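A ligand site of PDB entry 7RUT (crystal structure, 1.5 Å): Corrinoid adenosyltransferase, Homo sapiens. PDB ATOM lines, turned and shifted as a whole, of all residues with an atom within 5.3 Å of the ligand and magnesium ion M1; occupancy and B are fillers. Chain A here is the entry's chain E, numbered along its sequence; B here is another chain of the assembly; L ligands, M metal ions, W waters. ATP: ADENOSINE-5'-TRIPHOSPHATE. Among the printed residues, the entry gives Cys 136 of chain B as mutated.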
ATOM      1  N   ILE A   4      29.745 -15.960 -21.904  1.00  0.00           N
ATOM      2  CA  ILE A   4      28.566 -15.161 -21.581  1.00  0.00           C
ATOM      3  C   ILE A   4      28.272 -15.232 -20.085  1.00  0.00           C
ATOM      4  O   ILE A   4      27.790 -14.257 -19.493  1.00  0.00           O
ATOM      5  CB  ILE A   4      27.350 -15.622 -22.411  1.00  0.00           C
ATOM      6  CG1 ILE A   4      26.140 -14.729 -22.144  1.00  0.00           C
ATOM      7  CG2 ILE A   4      27.013 -17.066 -22.110  1.00  0.00           C
ATOM      8  CD1 ILE A   4      24.976 -15.051 -23.062  1.00  0.00           C
ATOM      9  N   TYR A   5      28.571 -16.368 -19.452  1.00  0.00           N
ATOM     10  CA  TYR A   5      28.426 -16.471 -17.998  1.00  0.00           C
ATOM     11  C   TYR A   5      29.751 -16.112 -17.352  1.00  0.00           C
ATOM     12  O   TYR A   5      30.704 -16.896 -17.351  1.00  0.00           O
ATOM     13  CB  TYR A   5      27.946 -17.869 -17.590  1.00  0.00           C
ATOM     14  CG  TYR A   5      28.688 -19.049 -18.183  1.00  0.00           C
ATOM     15  CD1 TYR A   5      28.347 -19.551 -19.431  1.00  0.00           C
ATOM     16  CD2 TYR A   5      29.704 -19.693 -17.479  1.00  0.00           C
ATOM     17  CE1 TYR A   5      29.016 -20.643 -19.979  1.00  0.00           C
ATOM     18  CE2 TYR A   5      30.362 -20.780 -17.999  1.00  0.00           C
ATOM     19  CZ  TYR A   5      30.021 -21.252 -19.253  1.00  0.00           C
ATOM     20  OH  TYR A   5      30.691 -22.341 -19.765  1.00  0.00           O
ATOM     21  N   THR A   6      29.830 -14.900 -16.809  1.00  0.00           N
ATOM     22  CA  THR A   6      31.028 -14.440 -16.123  1.00  0.00           C
ATOM     23  C   THR A   6      31.088 -14.928 -14.685  1.00  0.00           C
ATOM     24  O   THR A   6      32.180 -14.963 -14.095  1.00  0.00           O
ATOM     25  CB  THR A   6      31.096 -12.911 -16.123  1.00  0.00           C
ATOM     26  OG1 THR A   6      30.092 -12.380 -15.230  1.00  0.00           O
ATOM     27  CG2 THR A   6      30.892 -12.355 -17.533  1.00  0.00           C
ATOM     28  N   LYS A   7      29.936 -15.282 -14.108  1.00  0.00           N
ATOM     29  CA  LYS A   7      29.727 -15.683 -12.716  1.00  0.00           C
ATOM     30  C   LYS A   7      29.901 -14.510 -11.758  1.00  0.00           C
ATOM     31  O   LYS A   7      29.789 -14.715 -10.540  1.00  0.00           O
ATOM     32  CB  LYS A   7      30.634 -16.839 -12.301  1.00  0.00           C
ATOM     33  CG  LYS A   7      30.539 -18.015 -13.272  1.00  0.00           C
ATOM     34  CD  LYS A   7      31.197 -19.254 -12.717  1.00  0.00           C
ATOM     35  CE  LYS A   7      31.147 -20.399 -13.717  1.00  0.00           C
ATOM     36  NZ  LYS A   7      31.861 -21.592 -13.168  1.00  0.00           N
ATOM     37  N   THR A   8      30.156 -13.291 -12.249  1.00  0.00           N
ATOM     38  CA  THR A   8      30.225 -12.149 -11.346  1.00  0.00           C
ATOM     39  C   THR A   8      28.861 -11.811 -10.714  1.00  0.00           C
ATOM     40  O   THR A   8      28.825 -11.074  -9.733  1.00  0.00           O
ATOM     41  CB  THR A   8      30.808 -10.932 -12.092  1.00  0.00           C
ATOM     42  OG1 THR A   8      29.977 -10.579 -13.209  1.00  0.00           O
ATOM     43  CG2 THR A   8      32.211 -11.234 -12.612  1.00  0.00           C
ATOM     44  N   GLY A   9      27.760 -12.372 -11.229  1.00  0.00           N
ATOM     45  CA  GLY A   9      26.437 -12.246 -10.651  1.00  0.00           C
ATOM     46  C   GLY A   9      26.023 -13.399  -9.748  1.00  0.00           C
ATOM     47  O   GLY A   9      24.877 -13.398  -9.270  1.00  0.00           O
ATOM     48  N   ASP A  10      26.912 -14.364  -9.483  1.00  0.00           N
ATOM     49  CA  ASP A  10      26.529 -15.591  -8.794  1.00  0.00           C
ATOM     50  C   ASP A  10      26.350 -15.413  -7.282  1.00  0.00           C
ATOM     51  O   ASP A  10      25.887 -16.343  -6.625  1.00  0.00           O
ATOM     52  CB  ASP A  10      27.565 -16.686  -9.024  1.00  0.00           C
ATOM     53  CG  ASP A  10      27.324 -17.496 -10.295  1.00  0.00           C
ATOM     54  OD1 ASP A  10      26.334 -17.227 -11.020  1.00  0.00           O
ATOM     55  OD2 ASP A  10      28.117 -18.416 -10.552  1.00  0.00           O
ATOM     56  N   PHE A  13      24.737  -9.986  -6.622  1.00  0.00           N
ATOM     57  CA  PHE A  13      25.033  -8.585  -6.901  1.00  0.00           C
ATOM     58  C   PHE A  13      25.339  -8.413  -8.377  1.00  0.00           C
ATOM     59  O   PHE A  13      25.752  -9.351  -9.061  1.00  0.00           O
ATOM     60  CB  PHE A  13      26.218  -8.111  -6.038  1.00  0.00           C
ATOM     61  CG  PHE A  13      25.861  -8.002  -4.599  1.00  0.00           C
ATOM     62  CD1 PHE A  13      25.755  -9.139  -3.811  1.00  0.00           C
ATOM     63  CD2 PHE A  13      25.536  -6.770  -4.043  1.00  0.00           C
ATOM     64  CE1 PHE A  13      25.370  -9.055  -2.483  1.00  0.00           C
ATOM     65  CE2 PHE A  13      25.159  -6.676  -2.714  1.00  0.00           C
ATOM     66  CZ  PHE A  13      25.072  -7.809  -1.937  1.00  0.00           C
ATOM     67  N   SER A  14      25.110  -7.204  -8.886  1.00  0.00           N
ATOM     68  CA  SER A  14      25.437  -6.928 -10.284  1.00  0.00           C
ATOM     69  C   SER A  14      25.888  -5.479 -10.401  1.00  0.00           C
ATOM     70  O   SER A  14      25.917  -4.745  -9.413  1.00  0.00           O
ATOM     71  CB  SER A  14      24.230  -7.252 -11.192  1.00  0.00           C
ATOM     72  OG  SER A  14      24.634  -7.318 -12.553  1.00  0.00           O
ATOM     73  N   SER A  15      26.229  -5.068 -11.621  1.00  0.00           N
ATOM     74  CA  SER A  15      26.787  -3.752 -11.889  1.00  0.00           C
ATOM     75  C   SER A  15      25.787  -2.886 -12.640  1.00  0.00           C
ATOM     76  O   SER A  15      25.150  -3.346 -13.584  1.00  0.00           O
ATOM     77  CB  SER A  15      28.075  -3.862 -12.705  1.00  0.00           C
ATOM     78  OG  SER A  15      29.085  -4.540 -11.988  1.00  0.00           O
ATOM     79  N   THR A  16      25.674  -1.626 -12.222  1.00  0.00           N
ATOM     80  CA  THR A  16      24.968  -0.636 -13.021  1.00  0.00           C
ATOM     81  C   THR A  16      25.850  -0.194 -14.187  1.00  0.00           C
ATOM     82  O   THR A  16      27.021  -0.584 -14.301  1.00  0.00           O
ATOM     83  CB  THR A  16      24.583   0.582 -12.194  1.00  0.00           C
ATOM     84  OG1 THR A  16      25.763   1.319 -11.869  1.00  0.00           O
ATOM     85  CG2 THR A  16      23.836   0.177 -10.926  1.00  0.00           C
ATOM     86  N   ARG A  21      28.207  -1.457  -7.791  1.00  0.00           N
ATOM     87  CA  ARG A  21      27.645  -2.755  -7.416  1.00  0.00           C
ATOM     88  C   ARG A  21      26.395  -2.554  -6.549  1.00  0.00           C
ATOM     89  O   ARG A  21      26.425  -1.778  -5.588  1.00  0.00           O
ATOM     90  CB  ARG A  21      28.676  -3.602  -6.668  1.00  0.00           C
ATOM     91  CG  ARG A  21      29.923  -3.921  -7.498  1.00  0.00           C
ATOM     92  CD  ARG A  21      29.616  -4.826  -8.687  1.00  0.00           C
ATOM     93  NE  ARG A  21      29.405  -6.194  -8.241  1.00  0.00           N
ATOM     94  CZ  ARG A  21      29.087  -7.200  -9.051  1.00  0.00           C
ATOM     95  NH1 ARG A  21      28.928  -6.987 -10.356  1.00  0.00           N
ATOM     96  NH2 ARG A  21      28.926  -8.420  -8.543  1.00  0.00           N
ATOM     97  N   LYS A  24      20.923  -7.613  -6.617  1.00  0.00           N
ATOM     98  CA  LYS A  24      20.087  -7.775  -7.792  1.00  0.00           C
ATOM     99  C   LYS A  24      18.617  -7.462  -7.528  1.00  0.00           C
ATOM    100  O   LYS A  24      17.865  -7.248  -8.492  1.00  0.00           O
ATOM    101  CB  LYS A  24      20.232  -9.188  -8.347  1.00  0.00           C
ATOM    102  CG  LYS A  24      21.500  -9.378  -9.141  1.00  0.00           C
ATOM    103  CD  LYS A  24      21.623 -10.798  -9.642  1.00  0.00           C
ATOM    104  CE  LYS A  24      22.842 -10.930 -10.538  1.00  0.00           C
ATOM    105  NZ  LYS A  24      22.953 -12.270 -11.187  1.00  0.00           N
ATOM    106  N   PHE A  29      17.503  -2.614 -10.760  1.00  0.00           N
ATOM    107  CA  PHE A  29      17.396  -3.833 -11.556  1.00  0.00           C
ATOM    108  C   PHE A  29      15.954  -4.280 -11.713  1.00  0.00           C
ATOM    109  O   PHE A  29      15.600  -4.910 -12.718  1.00  0.00           O
ATOM    110  CB  PHE A  29      18.256  -4.936 -10.945  1.00  0.00           C
ATOM    111  CG  PHE A  29      19.711  -4.605 -10.927  1.00  0.00           C
ATOM    112  CD1 PHE A  29      20.351  -4.204 -12.085  1.00  0.00           C
ATOM    113  CD2 PHE A  29      20.431  -4.657  -9.738  1.00  0.00           C
ATOM    114  CE1 PHE A  29      21.714  -3.885 -12.078  1.00  0.00           C
ATOM    115  CE2 PHE A  29      21.782  -4.337  -9.725  1.00  0.00           C
ATOM    116  CZ  PHE A  29      22.425  -3.948 -10.891  1.00  0.00           C
ATOM    117  N   GLU A  30      15.106  -3.958 -10.739  1.00  0.00           N
ATOM    118  CA  GLU A  30      13.680  -4.226 -10.915  1.00  0.00           C
ATOM    119  C   GLU A  30      13.105  -3.418 -12.077  1.00  0.00           C
ATOM    120  O   GLU A  30      12.310  -3.936 -12.878  1.00  0.00           O
ATOM    121  CB  GLU A  30      12.930  -3.905  -9.618  1.00  0.00           C
ATOM    122  CG  GLU A  30      11.432  -4.140  -9.701  1.00  0.00           C
ATOM    123  CD  GLU A  30      11.047  -5.599  -9.868  1.00  0.00           C
ATOM    124  OE1 GLU A  30      11.882  -6.479  -9.656  1.00  0.00           O
ATOM    125  OE2 GLU A  30       9.866  -5.860 -10.159  1.00  0.00           O
ATOM    126  N   VAL A  32      14.961  -2.007 -14.661  1.00  0.00           N
ATOM    127  CA  VAL A  32      15.615  -2.473 -15.883  1.00  0.00           C
ATOM    128  C   VAL A  32      14.996  -3.795 -16.341  1.00  0.00           C
ATOM    129  O   VAL A  32      14.695  -3.996 -17.529  1.00  0.00           O
ATOM    130  CB  VAL A  32      17.142  -2.610 -15.656  1.00  0.00           C
ATOM    131  CG1 VAL A  32      17.814  -3.391 -16.803  1.00  0.00           C
ATOM    132  CG2 VAL A  32      17.799  -1.238 -15.469  1.00  0.00           C
ATOM    133  N   GLY A  33      14.805  -4.715 -15.390  1.00  0.00           N
ATOM    134  CA  GLY A  33      14.275  -6.019 -15.723  1.00  0.00           C
ATOM    135  C   GLY A  33      12.855  -5.966 -16.234  1.00  0.00           C
ATOM    136  O   GLY A  33      12.489  -6.693 -17.159  1.00  0.00           O
ATOM    137  N   CYS B 136      14.993 -13.675 -15.095  1.00  0.00           N
ATOM    138  CA  CYS B 136      15.689 -12.617 -14.354  1.00  0.00           C
ATOM    139  C   CYS B 136      14.849 -12.108 -13.194  1.00  0.00           C
ATOM    140  O   CYS B 136      15.381 -11.783 -12.125  1.00  0.00           O
ATOM    141  CB  CYS B 136      16.076 -11.482 -15.296  1.00  0.00           C
ATOM    142  SG  CYS B 136      17.384 -11.924 -16.466  1.00  0.00           S
ATOM    143  N   ARG B 137      13.532 -12.021 -13.393  1.00  0.00           N
ATOM    144  CA  ARG B 137      12.643 -11.631 -12.300  1.00  0.00           C
ATOM    145  C   ARG B 137      12.662 -12.679 -11.181  1.00  0.00           C
ATOM    146  O   ARG B 137      12.777 -12.326 -10.007  1.00  0.00           O
ATOM    147  CB  ARG B 137      11.229 -11.409 -12.831  1.00  0.00           C
ATOM    148  CG  ARG B 137      10.221 -10.987 -11.750  1.00  0.00           C
ATOM    149  CD  ARG B 137       9.117 -10.072 -12.312  1.00  0.00           C
ATOM    150  NE  ARG B 137       8.407 -10.615 -13.488  1.00  0.00           N
ATOM    151  CZ  ARG B 137       7.461 -11.542 -13.425  1.00  0.00           C
ATOM    152  NH1 ARG B 137       6.874 -11.946 -14.546  1.00  0.00           N
ATOM    153  NH2 ARG B 137       7.077 -12.078 -12.272  1.00  0.00           N
ATOM    154  N   GLU B 139      15.105 -14.638 -10.430  1.00  0.00           N
ATOM    155  CA  GLU B 139      16.366 -14.478  -9.729  1.00  0.00           C
ATOM    156  C   GLU B 139      16.302 -13.326  -8.726  1.00  0.00           C
ATOM    157  O   GLU B 139      16.777 -13.457  -7.583  1.00  0.00           O
ATOM    158  CB  GLU B 139      17.513 -14.252 -10.724  1.00  0.00           C
ATOM    159  CG  GLU B 139      18.866 -14.261 -10.027  1.00  0.00           C
ATOM    160  CD  GLU B 139      20.012 -13.819 -10.914  1.00  0.00           C
ATOM    161  OE1 GLU B 139      19.754 -13.330 -12.047  1.00  0.00           O
ATOM    162  OE2 GLU B 139      21.176 -13.966 -10.471  1.00  0.00           O
ATOM    163  N   ARG B 140      15.707 -12.197  -9.115  1.00  0.00           N
ATOM    164  CA  ARG B 140      15.574 -11.067  -8.193  1.00  0.00           C
ATOM    165  C   ARG B 140      14.771 -11.446  -6.952  1.00  0.00           C
ATOM    166  O   ARG B 140      15.011 -10.906  -5.870  1.00  0.00           O
ATOM    167  CB  ARG B 140      14.942  -9.840  -8.895  1.00  0.00           C
ATOM    168  CG  ARG B 140      15.815  -9.271 -10.021  1.00  0.00           C
ATOM    169  CD  ARG B 140      15.426  -7.861 -10.461  1.00  0.00           C
ATOM    170  NE  ARG B 140      14.031  -7.775 -10.903  1.00  0.00           N
ATOM    171  CZ  ARG B 140      13.592  -8.098 -12.112  1.00  0.00           C
ATOM    172  NH1 ARG B 140      14.433  -8.544 -13.041  1.00  0.00           N
ATOM    173  NH2 ARG B 140      12.300  -7.975 -12.385  1.00  0.00           N
ATOM    174  N   ASN B 160      20.588 -17.574 -12.303  1.00  0.00           N
ATOM    175  CA  ASN B 160      21.498 -16.711 -13.042  1.00  0.00           C
ATOM    176  C   ASN B 160      21.951 -17.387 -14.338  1.00  0.00           C
ATOM    177  O   ASN B 160      21.840 -16.824 -15.437  1.00  0.00           O
ATOM    178  CB  ASN B 160      22.714 -16.351 -12.174  1.00  0.00           C
ATOM    179  CG  ASN B 160      23.598 -15.270 -12.793  1.00  0.00           C
ATOM    180  OD1 ASN B 160      23.140 -14.422 -13.563  1.00  0.00           O
ATOM    181  ND2 ASN B 160      24.885 -15.304 -12.445  1.00  0.00           N
ATOM    182  N   ARG B 161      22.448 -18.617 -14.234  1.00  0.00           N
ATOM    183  CA  ARG B 161      22.914 -19.329 -15.423  1.00  0.00           C
ATOM    184  C   ARG B 161      21.776 -19.612 -16.393  1.00  0.00           C
ATOM    185  O   ARG B 161      21.989 -19.640 -17.617  1.00  0.00           O
ATOM    186  CB  ARG B 161      23.615 -20.624 -15.022  1.00  0.00           C
ATOM    187  CG  ARG B 161      24.659 -21.089 -16.030  1.00  0.00           C
ATOM    188  CD  ARG B 161      25.907 -20.224 -15.962  1.00  0.00           C
ATOM    189  NE  ARG B 161      26.703 -20.536 -14.777  1.00  0.00           N
ATOM    190  CZ  ARG B 161      26.798 -19.767 -13.702  1.00  0.00           C
ATOM    191  NH1 ARG B 161      26.159 -18.605 -13.638  1.00  0.00           N
ATOM    192  NH2 ARG B 161      27.559 -20.159 -12.680  1.00  0.00           N
ATOM    193  N   ASP B 164      21.158 -16.948 -19.007  1.00  0.00           N
ATOM    194  CA  ASP B 164      22.143 -17.024 -20.090  1.00  0.00           C
ATOM    195  C   ASP B 164      21.811 -18.148 -21.064  1.00  0.00           C
ATOM    196  O   ASP B 164      21.987 -17.992 -22.270  1.00  0.00           O
ATOM    197  CB  ASP B 164      23.547 -17.240 -19.531  1.00  0.00           C
ATOM    198  CG  ASP B 164      24.128 -16.002 -18.860  1.00  0.00           C
ATOM    199  OD1 ASP B 164      23.481 -14.932 -18.901  1.00  0.00           O
ATOM    200  OD2 ASP B 164      25.224 -16.123 -18.295  1.00  0.00           O
HETATM  201  PG  ATP L   1      26.714 -13.107 -14.857  1.00  0.00           P
HETATM  202  O1G ATP L   1      25.362 -13.558 -15.367  1.00  0.00           O
HETATM  203  O2G ATP L   1      27.160 -13.812 -13.606  1.00  0.00           O
HETATM  204  O3G ATP L   1      27.764 -13.098 -15.937  1.00  0.00           O
HETATM  205  PB  ATP L   1      25.301 -10.713 -14.024  1.00  0.00           P
HETATM  206  O1B ATP L   1      25.723  -9.666 -13.008  1.00  0.00           O
HETATM  207  O2B ATP L   1      24.186 -11.669 -13.688  1.00  0.00           O
HETATM  208  O3B ATP L   1      26.625 -11.527 -14.488  1.00  0.00           O
HETATM  209  PA  ATP L   1      24.235 -10.343 -16.732  1.00  0.00           P
HETATM  210  O1A ATP L   1      23.428 -11.593 -16.496  1.00  0.00           O
HETATM  211  O2A ATP L   1      25.313 -10.302 -17.807  1.00  0.00           O
HETATM  212  O3A ATP L   1      24.943  -9.845 -15.359  1.00  0.00           O
HETATM  213  O5' ATP L   1      23.189  -9.145 -16.962  1.00  0.00           O
HETATM  214  C5' ATP L   1      23.539  -7.992 -17.729  1.00  0.00           C
HETATM  215  C4' ATP L   1      23.129  -6.745 -16.946  1.00  0.00           C
HETATM  216  O4' ATP L   1      21.745  -6.804 -16.568  1.00  0.00           O
HETATM  217  C3' ATP L   1      23.895  -6.635 -15.640  1.00  0.00           C
HETATM  218  O3' ATP L   1      25.113  -5.939 -15.811  1.00  0.00           O
HETATM  219  C2' ATP L   1      22.930  -5.882 -14.739  1.00  0.00           C
HETATM  220  O2' ATP L   1      23.003  -4.492 -15.065  1.00  0.00           O
HETATM  221  C1' ATP L   1      21.580  -6.358 -15.208  1.00  0.00           C
HETATM  222  N9  ATP L   1      21.063  -7.548 -14.474  1.00  0.00           N
HETATM  223  C8  ATP L   1      21.746  -8.641 -14.088  1.00  0.00           C
HETATM  224  N7  ATP L   1      20.940  -9.550 -13.489  1.00  0.00           N
HETATM  225  C5  ATP L   1      19.695  -9.027 -13.498  1.00  0.00           C
HETATM  226  C6  ATP L   1      18.366  -9.481 -13.051  1.00  0.00           C
HETATM  227  N6  ATP L   1      18.230 -10.680 -12.440  1.00  0.00           N
HETATM  228  N1  ATP L   1      17.329  -8.641 -13.238  1.00  0.00           N
HETATM  229  C2  ATP L   1      17.482  -7.438 -13.847  1.00  0.00           C
HETATM  230  N3  ATP L   1      18.660  -6.972 -14.303  1.00  0.00           N
HETATM  231  C4  ATP L   1      19.776  -7.714 -14.153  1.00  0.00           C
HETATM  232 MG    MG M   1      23.388 -13.000 -14.964  1.00  0.00          MG
HETATM  233 MG    MG M   2      24.318 -11.447 -20.763  1.00  0.00          MG
HETATM  234  O   HOH W   1      21.492 -12.327 -14.391  1.00  0.00           O
HETATM  235  O   HOH W   2      27.803 -10.684 -17.669  1.00  0.00           O
HETATM  236  O   HOH W   3      22.676 -14.347 -16.338  1.00  0.00           O
HETATM  237  O   HOH W   4      27.373  -6.822 -14.323  1.00  0.00           O
HETATM  238  O   HOH W   5      20.713 -12.055 -17.428  1.00  0.00           O
HETATM  239  O   HOH W   6      28.082  -8.840 -12.307  1.00  0.00           O
HETATM  240  O   HOH W   7      25.416 -16.549 -15.636  1.00  0.00           O
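Magnesium ion M1 is bound by O2B of the ligand (2.0 Å). The side-chain amide oxygen (OD1) of Asn 160 of chain B is bound to magnesium ion M1 (2.0 Å). Magnesium ion M1 is bound by water W3 (2.1 Å). Magnesium ion M1 is bound by O1A of the ligand (2.1 Å). Magnesium ion M1 is bound by an oxygen (O1G) of the ligand, 2.1 Å away. Water W1 is bound to magnesium ion M1 (2.1 Å). Magnesium ion M1 has six donor atoms within binding distance.
Water W1 bridges N7 of the ligand and OE1 of Glu 139 of chain B. Water W3 lies within hydrogen-bond range of OD1 of Asp 164 of chain B and O of Asn 160 of chain B. Water W6 lies within hydrogen-bond range of an oxygen (O1B) of the ligand (2.6 Å), the side-chain hydroxyl of Thr 8 (2.7 Å) and the guanidinium group of Arg 21 (2.8 Å). Water W4 lies within hydrogen-bond range of an oxygen (O3') of the ligand (2.8 Å), the side-chain hydroxyl (OG) of Ser 14 (3.3 Å) and the backbone NH (N) of Ser 15 (3.4 Å). Water W7 lies within hydrogen-bond range of the side-chain carboxylate of Asp 164 of chain B (2.7 Å), the guanidinium group of Arg 161 of chain B (3.0 Å) and the side-chain amide nitrogen of Asn 160 of chain B (3.5 Å).
The side-chain carboxylate (OD1) of Asp 10 sits at hydrogen-bond distance from the side-chain amide nitrogen (ND2) of Asn 160 of chain B (2.8 Å). The side-chain amide oxygen (OD1) of Asn 160 of chain B lies close to the side-chain amino group (NZ) of Lys 24 (3.2 Å). The backbone carbonyl oxygen of Cys 136 of chain B sits close to the guanidinium group of Arg 140 of chain B (3.5 Å). The guanidinium group (NE) of Arg 140 of chain B lies within salt-bridge range of the side-chain carboxylate (OE1) of Glu 30, at 2.8 Å. The backbone carbonyl oxygen (O) of Thr 8 lies within hydrogen-bond range of the guanidinium group (NH2) of Arg 21 (2.9 Å). OG of Ser 15 sits at hydrogen-bond distance from NH1 of Arg 21 (2.9 Å). O of Phe 13 sits at hydrogen-bond distance from NH2 of Arg 21 (3.3 Å). O of Gly 9 lies within hydrogen-bond range of NZ of Lys 24 (2.9 Å).
Ile 4 touches the ligand (O to O3G, 3.7 Å). Tyr 5 touches the ligand (C to O3G, 3.9 Å). Phe 13 touches the ligand (O to O1B, 3.96 Å). Phe 29 touches the ligand (CE1 to O2', 3.3 Å). Gly 33 touches the ligand. Asp 164 of chain B touches the ligand (OD2 to O1G, 3.9 Å). Hydrophobic or aromatic side chains within 4 Å of the ligand: Phe 29. Of the 24 residues printed, 17 come within 4 Å of the ligand. Along chain A the residues within 4 Å of the ligand span positions 4 to 33.
An oxygen (O2') of the ligand lies within hydrogen-bond range of the backbone carbonyl oxygen (O) of Ser 15 (2.8 Å). OE1 of Glu 139 of chain B lies within hydrogen-bond range of N6 of the ligand, 3.1 Å away. The backbone NH (N) of Thr 8 lies within hydrogen-bond range of an oxygen (O2G) of the ligand (3.3 Å). The backbone NH (N) of Thr 6 sits at hydrogen-bond distance from an oxygen (O3G) of the ligand, 2.9 Å away. The side-chain hydroxyl (OG1) of Thr 6 lies within hydrogen-bond range of an oxygen (O3G) of the ligand (2.5 Å). NZ of Lys 24 sits close to O2B of the ligand. The backbone carbonyl oxygen (O) of Cys 136 of chain B sits at hydrogen-bond distance from a nitrogen (N6) of the ligand (3.1 Å). The backbone NH (N) of Lys 7 is in hydrogen-bond range of an oxygen (O2G) of the ligand (3.2 Å). OG of Ser 14 is in hydrogen-bond range of O1B of the ligand (2.6 Å). N1 of the ligand lies within hydrogen-bond range of NH1 of Arg 140 of chain B, at 2.9 Å. An oxygen (O2G) of the ligand sits at hydrogen-bond distance from the backbone NH (N) of Gly 9 (2.8 Å).
Lys 24 touches magnesium ion M1. Of the 24 residues printed, 2 come within 4 Å of magnesium ion M1.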
